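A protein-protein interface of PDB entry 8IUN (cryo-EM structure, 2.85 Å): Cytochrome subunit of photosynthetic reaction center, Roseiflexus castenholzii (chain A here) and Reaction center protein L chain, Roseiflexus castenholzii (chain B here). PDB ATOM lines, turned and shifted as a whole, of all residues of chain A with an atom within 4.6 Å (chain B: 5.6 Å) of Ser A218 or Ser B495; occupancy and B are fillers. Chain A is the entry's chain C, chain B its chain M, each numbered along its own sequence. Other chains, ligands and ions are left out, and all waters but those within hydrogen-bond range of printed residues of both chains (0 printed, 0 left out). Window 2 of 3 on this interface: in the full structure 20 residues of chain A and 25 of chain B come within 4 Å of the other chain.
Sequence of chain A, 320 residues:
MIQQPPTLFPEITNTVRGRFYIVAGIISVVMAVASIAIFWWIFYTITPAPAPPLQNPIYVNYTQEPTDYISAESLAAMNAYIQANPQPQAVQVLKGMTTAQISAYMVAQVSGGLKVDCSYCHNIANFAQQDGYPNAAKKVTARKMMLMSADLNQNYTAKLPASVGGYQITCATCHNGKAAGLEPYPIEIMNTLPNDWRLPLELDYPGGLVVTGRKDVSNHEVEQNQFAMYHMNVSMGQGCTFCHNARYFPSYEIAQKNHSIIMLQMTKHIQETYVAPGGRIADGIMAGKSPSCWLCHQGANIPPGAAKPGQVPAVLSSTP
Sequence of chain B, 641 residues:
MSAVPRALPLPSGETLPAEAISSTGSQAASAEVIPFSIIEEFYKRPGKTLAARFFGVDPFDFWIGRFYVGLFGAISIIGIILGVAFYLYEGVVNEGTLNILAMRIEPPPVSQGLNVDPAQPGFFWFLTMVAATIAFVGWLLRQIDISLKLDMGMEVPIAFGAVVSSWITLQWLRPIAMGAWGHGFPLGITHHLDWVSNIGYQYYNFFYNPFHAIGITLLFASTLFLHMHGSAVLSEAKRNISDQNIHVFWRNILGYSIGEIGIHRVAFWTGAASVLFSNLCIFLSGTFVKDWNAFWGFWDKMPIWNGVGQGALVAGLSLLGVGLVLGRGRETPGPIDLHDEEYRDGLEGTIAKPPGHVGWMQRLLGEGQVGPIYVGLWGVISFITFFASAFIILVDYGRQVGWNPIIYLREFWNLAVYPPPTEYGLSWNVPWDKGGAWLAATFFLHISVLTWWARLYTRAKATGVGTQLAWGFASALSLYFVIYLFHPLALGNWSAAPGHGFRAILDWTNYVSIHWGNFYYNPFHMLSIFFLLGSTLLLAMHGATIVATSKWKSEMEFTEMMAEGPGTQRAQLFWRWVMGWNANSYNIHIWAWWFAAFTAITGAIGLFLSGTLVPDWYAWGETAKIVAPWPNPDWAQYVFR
OG1 of Thr B422 is in hydrogen-bond range of OG of Ser B495 (3.3 Å). The side-chain amide nitrogen (ND2) of Asn B493 lies within hydrogen-bond range of the side-chain hydroxyl (OG) of Ser B495, 3.0 Å away. N of Ser A218 lies within hydrogen-bond range of OE1 of Glu A221.
Of chain A, only Ser A218 and Asn A219 come within 4 Å of Ser B495. Of the printed residues of chain A, Thr B422 touches Ser A218 and Glu A221. Of the printed residues of chain A, Asn B493 touches Ser A218. Ala B497 touches none of the printed residues of chain A. The nearest residue of chain B that does not touch Ser A218 is His B515 (4.1 Å).
Printed residues of chain B that touch a printed residue of chain A: Thr B422, Asn B493, Ser B495, Ala B496 and His B515. Hydrophobic or aromatic side chains of chain B within 4 Å of the printed part of chain A: His B515. Of the 6 printed residues of chain A, 4 touch a printed residue of chain B. Among the printed residues, no Asp or Glu carboxylate lies within 4 Å of a Lys or Arg side-chain nitrogen of the other chain.
The side-chain hydroxyl (OG1) of Thr B422 is in hydrogen-bond range of the side-chain carboxylate (OE1) of Glu A221, 3.5 Å away. The side-chain amide nitrogen of Asn B493 is in hydrogen-bond range of the side-chain hydroxyl of Ser A218. OG of Ser B495 sits at hydrogen-bond distance from OG of Ser A218.
O of Val A217 touches CE1 of His B515, at 3.2 Å. Ser A218 touches Thr B422 (CB to OG1, 3.3 Å). Ser A218 touches Ala B496 (OG to N, 3.7 Å). Asn A219 touches Ser B495.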
ATOM      1  N   VAL A 217     -20.790 -16.603 -13.354  1.00  0.00           N
ATOM      2  CA  VAL A 217     -20.480 -17.560 -12.302  1.00  0.00           C
ATOM      3  C   VAL A 217     -19.097 -17.204 -11.772  1.00  0.00           C
ATOM      4  O   VAL A 217     -18.285 -16.608 -12.481  1.00  0.00           O
ATOM      5  CB  VAL A 217     -20.579 -19.004 -12.863  1.00  0.00           C
ATOM      6  CG1 VAL A 217     -19.540 -19.939 -12.279  1.00  0.00           C
ATOM      7  CG2 VAL A 217     -21.965 -19.556 -12.631  1.00  0.00           C
ATOM      8  N   SER A 218     -18.841 -17.526 -10.508  1.00  0.00           N
ATOM      9  CA  SER A 218     -17.537 -17.258  -9.911  1.00  0.00           C
ATOM     10  C   SER A 218     -17.167 -18.433  -9.014  1.00  0.00           C
ATOM     11  O   SER A 218     -17.737 -19.523  -9.116  1.00  0.00           O
ATOM     12  CB  SER A 218     -17.538 -15.917  -9.173  1.00  0.00           C
ATOM     13  OG  SER A 218     -16.224 -15.408  -9.075  1.00  0.00           O
ATOM     14  N   ASN A 219     -16.184 -18.217  -8.136  1.00  0.00           N
ATOM     15  CA  ASN A 219     -15.597 -19.291  -7.339  1.00  0.00           C
ATOM     16  C   ASN A 219     -16.549 -19.859  -6.293  1.00  0.00           C
ATOM     17  O   ASN A 219     -16.338 -20.989  -5.837  1.00  0.00           O
ATOM     18  CB  ASN A 219     -14.323 -18.790  -6.663  1.00  0.00           C
ATOM     19  CG  ASN A 219     -13.156 -18.693  -7.621  1.00  0.00           C
ATOM     20  OD1 ASN A 219     -13.325 -18.755  -8.835  1.00  0.00           O
ATOM     21  ND2 ASN A 219     -11.963 -18.537  -7.077  1.00  0.00           N
ATOM     22  N   HIS A 220     -17.580 -19.111  -5.900  1.00  0.00           N
ATOM     23  CA  HIS A 220     -18.601 -19.635  -4.995  1.00  0.00           C
ATOM     24  C   HIS A 220     -19.336 -20.820  -5.626  1.00  0.00           C
ATOM     25  O   HIS A 220     -19.528 -21.872  -4.995  1.00  0.00           O
ATOM     26  CB  HIS A 220     -19.566 -18.498  -4.645  1.00  0.00           C
ATOM     27  CG  HIS A 220     -20.549 -18.827  -3.567  1.00  0.00           C
ATOM     28  ND1 HIS A 220     -21.847 -19.208  -3.834  1.00  0.00           N
ATOM     29  CD2 HIS A 220     -20.435 -18.804  -2.219  1.00  0.00           C
ATOM     30  CE1 HIS A 220     -22.483 -19.424  -2.698  1.00  0.00           C
ATOM     31  NE2 HIS A 220     -21.649 -19.185  -1.702  1.00  0.00           N
ATOM     32  N   GLU A 221     -19.710 -20.679  -6.897  1.00  0.00           N
ATOM     33  CA  GLU A 221     -20.387 -21.754  -7.611  1.00  0.00           C
ATOM     34  C   GLU A 221     -19.448 -22.920  -7.891  1.00  0.00           C
ATOM     35  O   GLU A 221     -19.872 -24.081  -7.876  1.00  0.00           O
ATOM     36  CB  GLU A 221     -20.982 -21.214  -8.909  1.00  0.00           C
ATOM     37  CG  GLU A 221     -22.126 -20.232  -8.716  1.00  0.00           C
ATOM     38  CD  GLU A 221     -21.666 -18.815  -8.412  1.00  0.00           C
ATOM     39  OE1 GLU A 221     -20.451 -18.588  -8.288  1.00  0.00           O
ATOM     40  OE2 GLU A 221     -22.527 -17.922  -8.298  1.00  0.00           O
ATOM     41  N   VAL A 222     -18.170 -22.640  -8.147  1.00  0.00           N
ATOM     42  CA  VAL A 222     -17.214 -23.719  -8.370  1.00  0.00           C
ATOM     43  C   VAL A 222     -17.013 -24.526  -7.094  1.00  0.00           C
ATOM     44  O   VAL A 222     -16.876 -25.755  -7.136  1.00  0.00           O
ATOM     45  CB  VAL A 222     -15.882 -23.163  -8.909  1.00  0.00           C
ATOM     46  CG1 VAL A 222     -14.952 -24.299  -9.283  1.00  0.00           C
ATOM     47  CG2 VAL A 222     -16.119 -22.265 -10.108  1.00  0.00           C
ATOM     48  N   PRO B 419     -13.998 -13.626   0.212  1.00  0.00           N
ATOM     49  CA  PRO B 419     -14.534 -12.402  -0.385  1.00  0.00           C
ATOM     50  C   PRO B 419     -16.042 -12.483  -0.528  1.00  0.00           C
ATOM     51  O   PRO B 419     -16.618 -13.578  -0.481  1.00  0.00           O
ATOM     52  CB  PRO B 419     -13.839 -12.348  -1.753  1.00  0.00           C
ATOM     53  CG  PRO B 419     -13.355 -13.703  -2.001  1.00  0.00           C
ATOM     54  CD  PRO B 419     -13.056 -14.306  -0.687  1.00  0.00           C
ATOM     55  N   PRO B 420     -16.718 -11.348  -0.686  1.00  0.00           N
ATOM     56  CA  PRO B 420     -18.177 -11.365  -0.809  1.00  0.00           C
ATOM     57  C   PRO B 420     -18.621 -12.197  -1.997  1.00  0.00           C
ATOM     58  O   PRO B 420     -17.939 -12.231  -3.031  1.00  0.00           O
ATOM     59  CB  PRO B 420     -18.536  -9.882  -0.994  1.00  0.00           C
ATOM     60  CG  PRO B 420     -17.270  -9.195  -1.289  1.00  0.00           C
ATOM     61  CD  PRO B 420     -16.195  -9.975  -0.630  1.00  0.00           C
ATOM     62  N   PRO B 421     -19.760 -12.893  -1.885  1.00  0.00           N
ATOM     63  CA  PRO B 421     -20.224 -13.753  -2.984  1.00  0.00           C
ATOM     64  C   PRO B 421     -20.578 -13.002  -4.259  1.00  0.00           C
ATOM     65  O   PRO B 421     -20.515 -11.772  -4.309  1.00  0.00           O
ATOM     66  CB  PRO B 421     -21.455 -14.444  -2.386  1.00  0.00           C
ATOM     67  CG  PRO B 421     -21.844 -13.617  -1.223  1.00  0.00           C
ATOM     68  CD  PRO B 421     -20.584 -13.060  -0.678  1.00  0.00           C
ATOM     69  N   THR B 422     -20.953 -13.748  -5.300  1.00  0.00           N
ATOM     70  CA  THR B 422     -21.127 -13.175  -6.630  1.00  0.00           C
ATOM     71  C   THR B 422     -22.385 -12.322  -6.746  1.00  0.00           C
ATOM     72  O   THR B 422     -22.470 -11.493  -7.657  1.00  0.00           O
ATOM     73  CB  THR B 422     -21.153 -14.295  -7.673  1.00  0.00           C
ATOM     74  OG1 THR B 422     -20.164 -15.274  -7.342  1.00  0.00           O
ATOM     75  CG2 THR B 422     -20.854 -13.760  -9.059  1.00  0.00           C
ATOM     76  N   ASN B 493     -16.305  -8.862  -9.982  1.00  0.00           N
ATOM     77  CA  ASN B 493     -16.726  -9.351  -8.677  1.00  0.00           C
ATOM     78  C   ASN B 493     -15.504  -9.629  -7.813  1.00  0.00           C
ATOM     79  O   ASN B 493     -14.430  -9.955  -8.319  1.00  0.00           O
ATOM     80  CB  ASN B 493     -17.593 -10.610  -8.797  1.00  0.00           C
ATOM     81  CG  ASN B 493     -16.876 -11.750  -9.478  1.00  0.00           C
ATOM     82  OD1 ASN B 493     -15.858 -11.556 -10.130  1.00  0.00           O
ATOM     83  ND2 ASN B 493     -17.405 -12.949  -9.329  1.00  0.00           N
ATOM     84  N   TRP B 494     -15.683  -9.502  -6.497  1.00  0.00           N
ATOM     85  CA  TRP B 494     -14.600  -9.751  -5.555  1.00  0.00           C
ATOM     86  C   TRP B 494     -14.366 -11.227  -5.283  1.00  0.00           C
ATOM     87  O   TRP B 494     -13.296 -11.580  -4.782  1.00  0.00           O
ATOM     88  CB  TRP B 494     -14.867  -9.053  -4.221  1.00  0.00           C
ATOM     89  CG  TRP B 494     -14.702  -7.575  -4.250  1.00  0.00           C
ATOM     90  CD1 TRP B 494     -15.641  -6.645  -3.944  1.00  0.00           C
ATOM     91  CD2 TRP B 494     -13.519  -6.851  -4.602  1.00  0.00           C
ATOM     92  NE1 TRP B 494     -15.123  -5.387  -4.083  1.00  0.00           N
ATOM     93  CE2 TRP B 494     -13.820  -5.485  -4.486  1.00  0.00           C
ATOM     94  CE3 TRP B 494     -12.234  -7.228  -5.005  1.00  0.00           C
ATOM     95  CZ2 TRP B 494     -12.888  -4.495  -4.757  1.00  0.00           C
ATOM     96  CZ3 TRP B 494     -11.315  -6.245  -5.275  1.00  0.00           C
ATOM     97  CH2 TRP B 494     -11.645  -4.892  -5.153  1.00  0.00           C
ATOM     98  N   SER B 495     -15.327 -12.094  -5.591  1.00  0.00           N
ATOM     99  CA  SER B 495     -15.187 -13.514  -5.296  1.00  0.00           C
ATOM    100  C   SER B 495     -14.233 -14.225  -6.243  1.00  0.00           C
ATOM    101  O   SER B 495     -14.008 -15.427  -6.075  1.00  0.00           O
ATOM    102  CB  SER B 495     -16.551 -14.197  -5.328  1.00  0.00           C
ATOM    103  OG  SER B 495     -17.131 -14.091  -6.606  1.00  0.00           O
ATOM    104  N   ALA B 496     -13.677 -13.522  -7.225  1.00  0.00           N
ATOM    105  CA  ALA B 496     -12.658 -14.072  -8.104  1.00  0.00           C
ATOM    106  C   ALA B 496     -11.278 -14.099  -7.467  1.00  0.00           C
ATOM    107  O   ALA B 496     -10.347 -14.635  -8.073  1.00  0.00           O
ATOM    108  CB  ALA B 496     -12.600 -13.267  -9.402  1.00  0.00           C
ATOM    109  N   ALA B 497     -11.121 -13.530  -6.269  1.00  0.00           N
ATOM    110  CA  ALA B 497      -9.938 -13.337  -5.451  1.00  0.00           C
ATOM    111  C   ALA B 497      -9.829 -14.419  -4.382  1.00  0.00           C
ATOM    112  O   ALA B 497     -10.835 -15.003  -3.977  1.00  0.00           O
ATOM    113  CB  ALA B 497      -9.976 -11.961  -4.787  1.00  0.00           C
ATOM    114  N   HIS B 515     -12.435 -23.353 -13.659  1.00  0.00           N
ATOM    115  CA  HIS B 515     -13.409 -22.420 -14.222  1.00  0.00           C
ATOM    116  C   HIS B 515     -13.098 -22.088 -15.676  1.00  0.00           C
ATOM    117  O   HIS B 515     -13.979 -22.143 -16.539  1.00  0.00           O
ATOM    118  CB  HIS B 515     -13.435 -21.148 -13.376  1.00  0.00           C
ATOM    119  CG  HIS B 515     -14.586 -20.235 -13.667  1.00  0.00           C
ATOM    120  ND1 HIS B 515     -14.790 -19.063 -12.974  1.00  0.00           N
ATOM    121  CD2 HIS B 515     -15.594 -20.320 -14.564  1.00  0.00           C
ATOM    122  CE1 HIS B 515     -15.872 -18.465 -13.434  1.00  0.00           C
ATOM    123  NE2 HIS B 515     -16.380 -19.208 -14.398  1.00  0.00           N
